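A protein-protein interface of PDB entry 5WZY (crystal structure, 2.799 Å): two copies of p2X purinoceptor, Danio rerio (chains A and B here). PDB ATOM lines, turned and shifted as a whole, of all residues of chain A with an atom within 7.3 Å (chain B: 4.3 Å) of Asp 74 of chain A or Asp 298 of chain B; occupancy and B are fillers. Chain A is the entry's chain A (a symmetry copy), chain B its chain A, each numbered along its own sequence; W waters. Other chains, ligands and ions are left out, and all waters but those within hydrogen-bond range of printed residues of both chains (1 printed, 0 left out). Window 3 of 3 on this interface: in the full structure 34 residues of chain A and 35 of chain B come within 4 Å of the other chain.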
ATOM      1  N   SER A  40     -14.020 -22.680 -17.585  1.00  0.00           N
ATOM      2  CA  SER A  40     -14.334 -23.993 -17.014  1.00  0.00           C
ATOM      3  C   SER A  40     -14.810 -23.921 -15.571  1.00  0.00           C
ATOM      4  O   SER A  40     -14.455 -23.011 -14.830  1.00  0.00           O
ATOM      5  CB  SER A  40     -13.112 -24.930 -17.129  1.00  0.00           C
ATOM      6  OG  SER A  40     -13.030 -25.884 -16.076  1.00  0.00           O
ATOM      7  N   SER A  41     -15.627 -24.886 -15.186  1.00  0.00           N
ATOM      8  CA  SER A  41     -15.980 -25.089 -13.793  1.00  0.00           C
ATOM      9  C   SER A  41     -16.047 -26.598 -13.520  1.00  0.00           C
ATOM     10  O   SER A  41     -16.640 -27.354 -14.300  1.00  0.00           O
ATOM     11  CB  SER A  41     -17.312 -24.397 -13.469  1.00  0.00           C
ATOM     12  OG  SER A  41     -17.970 -24.998 -12.361  1.00  0.00           O
ATOM     13  N   VAL A  42     -15.420 -27.050 -12.437  1.00  0.00           N
ATOM     14  CA  VAL A  42     -15.535 -28.461 -12.079  1.00  0.00           C
ATOM     15  C   VAL A  42     -16.078 -28.686 -10.666  1.00  0.00           C
ATOM     16  O   VAL A  42     -15.832 -27.897  -9.770  1.00  0.00           O
ATOM     17  CB  VAL A  42     -14.210 -29.237 -12.303  1.00  0.00           C
ATOM     18  CG1 VAL A  42     -13.330 -28.490 -13.272  1.00  0.00           C
ATOM     19  CG2 VAL A  42     -13.478 -29.467 -10.995  1.00  0.00           C
ATOM     20  N   THR A  43     -16.848 -29.759 -10.496  1.00  0.00           N
ATOM     21  CA  THR A  43     -17.248 -30.258  -9.182  1.00  0.00           C
ATOM     22  C   THR A  43     -16.874 -31.738  -9.135  1.00  0.00           C
ATOM     23  O   THR A  43     -16.819 -32.388 -10.170  1.00  0.00           O
ATOM     24  CB  THR A  43     -18.769 -30.070  -8.923  1.00  0.00           C
ATOM     25  OG1 THR A  43     -19.531 -30.852  -9.851  1.00  0.00           O
ATOM     26  CG2 THR A  43     -19.164 -28.608  -9.060  1.00  0.00           C
ATOM     27  N   GLN A  72     -15.460 -30.110   0.508  1.00  0.00           N
ATOM     28  CA  GLN A  72     -15.590 -29.450  -0.782  1.00  0.00           C
ATOM     29  C   GLN A  72     -14.472 -28.423  -1.034  1.00  0.00           C
ATOM     30  O   GLN A  72     -14.169 -27.597  -0.173  1.00  0.00           O
ATOM     31  CB  GLN A  72     -16.975 -28.811  -0.871  1.00  0.00           C
ATOM     32  CG  GLN A  72     -17.146 -27.921  -2.046  1.00  0.00           C
ATOM     33  CD  GLN A  72     -16.916 -26.461  -1.736  1.00  0.00           C
ATOM     34  OE1 GLN A  72     -17.237 -25.987  -0.645  1.00  0.00           O
ATOM     35  NE2 GLN A  72     -16.347 -25.732  -2.699  1.00  0.00           N
ATOM     36  N   GLU A  73     -13.858 -28.490  -2.211  1.00  0.00           N
ATOM     37  CA  GLU A  73     -12.903 -27.478  -2.667  1.00  0.00           C
ATOM     38  C   GLU A  73     -13.251 -27.107  -4.100  1.00  0.00           C
ATOM     39  O   GLU A  73     -14.021 -27.801  -4.752  1.00  0.00           O
ATOM     40  CB  GLU A  73     -11.457 -27.997  -2.647  1.00  0.00           C
ATOM     41  CG  GLU A  73     -10.966 -28.560  -1.323  1.00  0.00           C
ATOM     42  CD  GLU A  73      -9.502 -28.950  -1.380  1.00  0.00           C
ATOM     43  OE1 GLU A  73      -9.181 -30.138  -1.112  1.00  0.00           O
ATOM     44  OE2 GLU A  73      -8.672 -28.063  -1.699  1.00  0.00           O
ATOM     45  N   ASP A  74     -12.673 -26.030  -4.610  1.00  0.00           N
ATOM     46  CA  ASP A  74     -12.946 -25.639  -5.983  1.00  0.00           C
ATOM     47  C   ASP A  74     -11.900 -26.282  -6.878  1.00  0.00           C
ATOM     48  O   ASP A  74     -10.728 -25.906  -6.845  1.00  0.00           O
ATOM     49  CB  ASP A  74     -12.938 -24.106  -6.092  1.00  0.00           C
ATOM     50  CG  ASP A  74     -12.935 -23.595  -7.536  1.00  0.00           C
ATOM     51  OD1 ASP A  74     -13.314 -24.344  -8.466  1.00  0.00           O
ATOM     52  OD2 ASP A  74     -12.563 -22.413  -7.740  1.00  0.00           O
ATOM     53  N   GLY A  75     -12.331 -27.255  -7.683  1.00  0.00           N
ATOM     54  CA  GLY A  75     -11.429 -27.956  -8.594  1.00  0.00           C
ATOM     55  C   GLY A  75     -10.193 -28.618  -7.978  1.00  0.00           C
ATOM     56  O   GLY A  75      -9.091 -28.574  -8.535  1.00  0.00           O
ATOM     57  N   SER A  76     -10.378 -29.184  -6.790  1.00  0.00           N
ATOM     58  CA  SER A  76      -9.359 -29.957  -6.105  1.00  0.00           C
ATOM     59  C   SER A  76     -10.050 -30.892  -5.114  1.00  0.00           C
ATOM     60  O   SER A  76     -11.099 -30.548  -4.565  1.00  0.00           O
ATOM     61  CB  SER A  76      -8.408 -29.007  -5.384  1.00  0.00           C
ATOM     62  OG  SER A  76      -7.464 -29.718  -4.619  1.00  0.00           O
ATOM     63  N   PHE A  77      -9.495 -32.072  -4.883  1.00  0.00           N
ATOM     64  CA  PHE A  77     -10.018 -32.917  -3.824  1.00  0.00           C
ATOM     65  C   PHE A  77      -8.923 -33.734  -3.143  1.00  0.00           C
ATOM     66  O   PHE A  77      -8.028 -34.274  -3.801  1.00  0.00           O
ATOM     67  CB  PHE A  77     -11.185 -33.796  -4.299  1.00  0.00           C
ATOM     68  CG  PHE A  77     -10.843 -34.778  -5.409  1.00  0.00           C
ATOM     69  CD1 PHE A  77     -10.899 -34.396  -6.745  1.00  0.00           C
ATOM     70  CD2 PHE A  77     -10.544 -36.106  -5.119  1.00  0.00           C
ATOM     71  CE1 PHE A  77     -10.609 -35.310  -7.781  1.00  0.00           C
ATOM     72  CE2 PHE A  77     -10.257 -37.017  -6.149  1.00  0.00           C
ATOM     73  CZ  PHE A  77     -10.289 -36.610  -7.483  1.00  0.00           C
ATOM     74  N   ASP A 298      -5.504 -32.504  -8.114  1.00  0.00           N
ATOM     75  CA  ASP A 298      -5.743 -31.233  -8.784  1.00  0.00           C
ATOM     76  C   ASP A 298      -6.390 -31.397 -10.155  1.00  0.00           C
ATOM     77  O   ASP A 298      -5.801 -31.978 -11.073  1.00  0.00           O
ATOM     78  CB  ASP A 298      -4.430 -30.489  -8.955  1.00  0.00           C
ATOM     79  CG  ASP A 298      -4.294 -29.336  -7.992  1.00  0.00           C
ATOM     80  OD1 ASP A 298      -3.769 -29.561  -6.867  1.00  0.00           O
ATOM     81  OD2 ASP A 298      -4.733 -28.213  -8.361  1.00  0.00           O
ATOM     82  N   VAL A 299      -7.599 -30.881 -10.306  1.00  0.00           N
ATOM     83  CA  VAL A 299      -8.243 -30.898 -11.609  1.00  0.00           C
ATOM     84  C   VAL A 299      -7.929 -29.591 -12.328  1.00  0.00           C
ATOM     85  O   VAL A 299      -8.298 -28.517 -11.850  1.00  0.00           O
ATOM     86  CB  VAL A 299      -9.755 -31.086 -11.479  1.00  0.00           C
ATOM     87  CG1 VAL A 299     -10.412 -31.153 -12.857  1.00  0.00           C
ATOM     88  CG2 VAL A 299     -10.046 -32.344 -10.683  1.00  0.00           C
ATOM     89  N   GLU B  73     -12.775 -19.991   1.998  1.00  0.00           N
ATOM     90  CA  GLU B  73     -12.067 -20.435   0.795  1.00  0.00           C
ATOM     91  C   GLU B  73     -11.433 -19.219   0.139  1.00  0.00           C
ATOM     92  O   GLU B  73     -11.763 -18.089   0.475  1.00  0.00           O
ATOM     93  CB  GLU B  73     -13.014 -21.087  -0.224  1.00  0.00           C
ATOM     94  CG  GLU B  73     -13.860 -22.241   0.290  1.00  0.00           C
ATOM     95  CD  GLU B  73     -14.682 -22.878  -0.813  1.00  0.00           C
ATOM     96  OE1 GLU B  73     -15.934 -22.926  -0.685  1.00  0.00           O
ATOM     97  OE2 GLU B  73     -14.070 -23.327  -1.814  1.00  0.00           O
ATOM     98  N   GLY B  75     -11.424 -16.842  -2.699  1.00  0.00           N
ATOM     99  CA  GLY B  75     -12.258 -16.411  -3.819  1.00  0.00           C
ATOM    100  C   GLY B  75     -13.346 -17.379  -4.291  1.00  0.00           C
ATOM    101  O   GLY B  75     -13.584 -17.547  -5.492  1.00  0.00           O
ATOM    102  N   VAL B 230     -23.648 -24.044  -9.487  1.00  0.00           N
ATOM    103  CA  VAL B 230     -22.466 -23.189  -9.429  1.00  0.00           C
ATOM    104  C   VAL B 230     -22.724 -21.794 -10.030  1.00  0.00           C
ATOM    105  O   VAL B 230     -23.116 -21.691 -11.189  1.00  0.00           O
ATOM    106  CB  VAL B 230     -21.304 -23.832 -10.195  1.00  0.00           C
ATOM    107  CG1 VAL B 230     -20.014 -23.050  -9.948  1.00  0.00           C
ATOM    108  CG2 VAL B 230     -21.155 -25.280  -9.794  1.00  0.00           C
ATOM    109  N   MET B 231     -22.494 -20.731  -9.256  1.00  0.00           N
ATOM    110  CA  MET B 231     -22.735 -19.352  -9.721  1.00  0.00           C
ATOM    111  C   MET B 231     -21.453 -18.582  -9.858  1.00  0.00           C
ATOM    112  O   MET B 231     -20.674 -18.500  -8.918  1.00  0.00           O
ATOM    113  CB  MET B 231     -23.644 -18.582  -8.757  1.00  0.00           C
ATOM    114  CG  MET B 231     -25.125 -18.898  -8.884  1.00  0.00           C
ATOM    115  SD  MET B 231     -25.866 -18.510 -10.498  1.00  0.00           S
ATOM    116  CE  MET B 231     -25.208 -16.858 -10.779  1.00  0.00           C
ATOM    117  N   GLY B 232     -21.196 -18.044 -11.033  1.00  0.00           N
ATOM    118  CA  GLY B 232     -20.074 -17.138 -11.185  1.00  0.00           C
ATOM    119  C   GLY B 232     -20.383 -15.680 -10.906  1.00  0.00           C
ATOM    120  O   GLY B 232     -21.415 -15.157 -11.336  1.00  0.00           O
ATOM    121  N   VAL B 233     -19.449 -15.011 -10.247  1.00  0.00           N
ATOM    122  CA  VAL B 233     -19.499 -13.568 -10.052  1.00  0.00           C
ATOM    123  C   VAL B 233     -18.228 -12.974 -10.669  1.00  0.00           C
ATOM    124  O   VAL B 233     -17.132 -13.176 -10.139  1.00  0.00           O
ATOM    125  CB  VAL B 233     -19.555 -13.222  -8.541  1.00  0.00           C
ATOM    126  CG1 VAL B 233     -19.329 -11.749  -8.305  1.00  0.00           C
ATOM    127  CG2 VAL B 233     -20.863 -13.660  -7.940  1.00  0.00           C
ATOM    128  N   LEU B 257     -22.726 -20.977 -13.844  1.00  0.00           N
ATOM    129  CA  LEU B 257     -21.612 -21.762 -14.395  1.00  0.00           C
ATOM    130  C   LEU B 257     -21.850 -23.240 -14.799  1.00  0.00           C
ATOM    131  O   LEU B 257     -21.231 -23.731 -15.749  1.00  0.00           O
ATOM    132  CB  LEU B 257     -20.409 -21.671 -13.463  1.00  0.00           C
ATOM    133  CG  LEU B 257     -19.853 -20.265 -13.449  1.00  0.00           C
ATOM    134  CD1 LEU B 257     -18.642 -20.178 -12.544  1.00  0.00           C
ATOM    135  CD2 LEU B 257     -19.520 -19.864 -14.870  1.00  0.00           C
ATOM    136  N   ARG B 296     -22.320 -23.137  -4.997  1.00  0.00           N
ATOM    137  CA  ARG B 296     -20.980 -22.610  -4.881  1.00  0.00           C
ATOM    138  C   ARG B 296     -20.928 -21.282  -5.640  1.00  0.00           C
ATOM    139  O   ARG B 296     -21.325 -21.230  -6.801  1.00  0.00           O
ATOM    140  CB  ARG B 296     -19.980 -23.587  -5.489  1.00  0.00           C
ATOM    141  CG  ARG B 296     -18.564 -23.328  -5.022  1.00  0.00           C
ATOM    142  CD  ARG B 296     -17.597 -23.195  -6.150  1.00  0.00           C
ATOM    143  NE  ARG B 296     -17.306 -24.513  -6.664  1.00  0.00           N
ATOM    144  CZ  ARG B 296     -16.936 -24.771  -7.913  1.00  0.00           C
ATOM    145  NH1 ARG B 296     -16.793 -23.791  -8.806  1.00  0.00           N
ATOM    146  NH2 ARG B 296     -16.710 -26.026  -8.269  1.00  0.00           N
ATOM    147  N   PHE B 297     -20.459 -20.214  -4.999  1.00  0.00           N
ATOM    148  CA  PHE B 297     -20.261 -18.937  -5.691  1.00  0.00           C
ATOM    149  C   PHE B 297     -18.792 -18.696  -6.028  1.00  0.00           C
ATOM    150  O   PHE B 297     -17.970 -18.510  -5.142  1.00  0.00           O
ATOM    151  CB  PHE B 297     -20.790 -17.777  -4.856  1.00  0.00           C
ATOM    152  CG  PHE B 297     -22.290 -17.733  -4.758  1.00  0.00           C
ATOM    153  CD1 PHE B 297     -22.967 -18.524  -3.841  1.00  0.00           C
ATOM    154  CD2 PHE B 297     -23.027 -16.897  -5.574  1.00  0.00           C
ATOM    155  CE1 PHE B 297     -24.360 -18.487  -3.750  1.00  0.00           C
ATOM    156  CE2 PHE B 297     -24.431 -16.863  -5.489  1.00  0.00           C
ATOM    157  CZ  PHE B 297     -25.088 -17.658  -4.578  1.00  0.00           C
ATOM    158  N   ASP B 298     -18.464 -18.708  -7.315  1.00  0.00           N
ATOM    159  CA  ASP B 298     -17.111 -18.410  -7.762  1.00  0.00           C
ATOM    160  C   ASP B 298     -16.894 -16.928  -8.051  1.00  0.00           C
ATOM    161  O   ASP B 298     -17.514 -16.356  -8.954  1.00  0.00           O
ATOM    162  CB  ASP B 298     -16.804 -19.197  -9.025  1.00  0.00           C
ATOM    163  CG  ASP B 298     -15.880 -20.361  -8.764  1.00  0.00           C
ATOM    164  OD1 ASP B 298     -16.394 -21.471  -8.458  1.00  0.00           O
ATOM    165  OD2 ASP B 298     -14.639 -20.151  -8.850  1.00  0.00           O
ATOM    166  N   VAL B 299     -16.008 -16.300  -7.294  1.00  0.00           N
ATOM    167  CA  VAL B 299     -15.663 -14.916  -7.571  1.00  0.00           C
ATOM    168  C   VAL B 299     -14.443 -14.889  -8.485  1.00  0.00           C
ATOM    169  O   VAL B 299     -13.375 -15.372  -8.108  1.00  0.00           O
ATOM    170  CB  VAL B 299     -15.378 -14.146  -6.280  1.00  0.00           C
ATOM    171  CG1 VAL B 299     -15.065 -12.681  -6.582  1.00  0.00           C
ATOM    172  CG2 VAL B 299     -16.567 -14.260  -5.345  1.00  0.00           C
ATOM    173  N   MET B 300     -14.615 -14.337  -9.688  1.00  0.00           N
ATOM    174  CA  MET B 300     -13.544 -14.231 -10.681  1.00  0.00           C
ATOM    175  C   MET B 300     -13.246 -12.778 -11.007  1.00  0.00           C
ATOM    176  O   MET B 300     -14.137 -12.044 -11.400  1.00  0.00           O
ATOM    177  CB  MET B 300     -13.953 -14.952 -11.962  1.00  0.00           C
ATOM    178  CG  MET B 300     -14.167 -16.453 -11.794  1.00  0.00           C
ATOM    179  SD  MET B 300     -15.204 -17.157 -13.093  1.00  0.00           S
ATOM    180  CE  MET B 300     -16.681 -16.131 -12.929  1.00  0.00           C
HETATM  181  O   HOH W   1     -12.175 -20.956  -9.624  1.00  0.00           O
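The side-chain carboxylate (OE1) of Glu 73 of chain B sits close to the side-chain amide oxygen (OE1) of Gln 72 of chain A, 3.3 Å away. NH2 of Arg 296 of chain B sits at hydrogen-bond distance from O of Val 42 of chain A, 2.6 Å away. NH1 of Arg 296 of chain B lies within salt-bridge range of OD1 of Asp 74 of chain A. The side-chain carboxylate of Asp 298 of chain B sits close to the side-chain carboxylate of Asp 74 of chain A, at 3.3 Å.
Positions printed for both chains: 73, 75, 298 and 299.
Among the printed residues, merely in contact across the chains: Thr 43 of chain A with Arg 296 of chain B, Ser 41 of chain A with Val 230 of chain B, Ser 41 of chain A with Arg 296 of chain B and Thr 43 of chain A with Val 230 of chain B.
The backbone carbonyl oxygen (O) of Val 230 of chain B is in hydrogen-bond range of the backbone NH (N) of Leu 257 of chain B (2.8 Å). The backbone NH (N) of Met 231 of chain B sits at hydrogen-bond distance from the backbone carbonyl oxygen (O) of Arg 296 of chain B (2.8 Å). N of Asp 298 of chain B sits at hydrogen-bond distance from O of Met 231 of chain B, 2.7 Å away. N of Val 233 of chain B is in hydrogen-bond range of O of Asp 298 of chain B, at 2.7 Å. The side-chain carboxylate (OD1) of Asp 298 of chain B is in salt-bridge range of the guanidinium group (NE) of Arg 296 of chain B.
Printed residues of chain A that touch a printed residue of chain B: Ser 41, Val 42, Thr 43, Gln 72 and Asp 74. Along chain A the printed residues that touch a printed residue of chain B span positions 41 to 74. Hydrophobic or aromatic side chains of chain B that line the printed part of chain A: Val 230. Among the printed residues, Asp or Glu carboxylates within 4 Å of a Lys or Arg side-chain nitrogen of the other chain: Asp 74 of chain A with Arg 296 of chain B (3.5 Å).
Water W1 lies within hydrogen-bond range of the side-chain carboxylate (OD2) of Asp 74 of chain A and the side-chain carboxylate (OD2) of Asp 298 of chain B.
Of the printed residues of chain B, Val 42 of chain A touches Arg 296 (2.6 Å). Asp 74 of chain A touches just these residues of chain B: Arg 296 (3.5 Å) and Asp 298 (3.3 Å). Printed residues of chain A within 4 Å of Glu 73 of chain B: Gln 72 (3.3 Å). Gly 75 of chain B touches none of the printed residues of chain A. Printed residues of chain A within 4 Å of Val 230 of chain B: Ser 41 and Thr 43.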
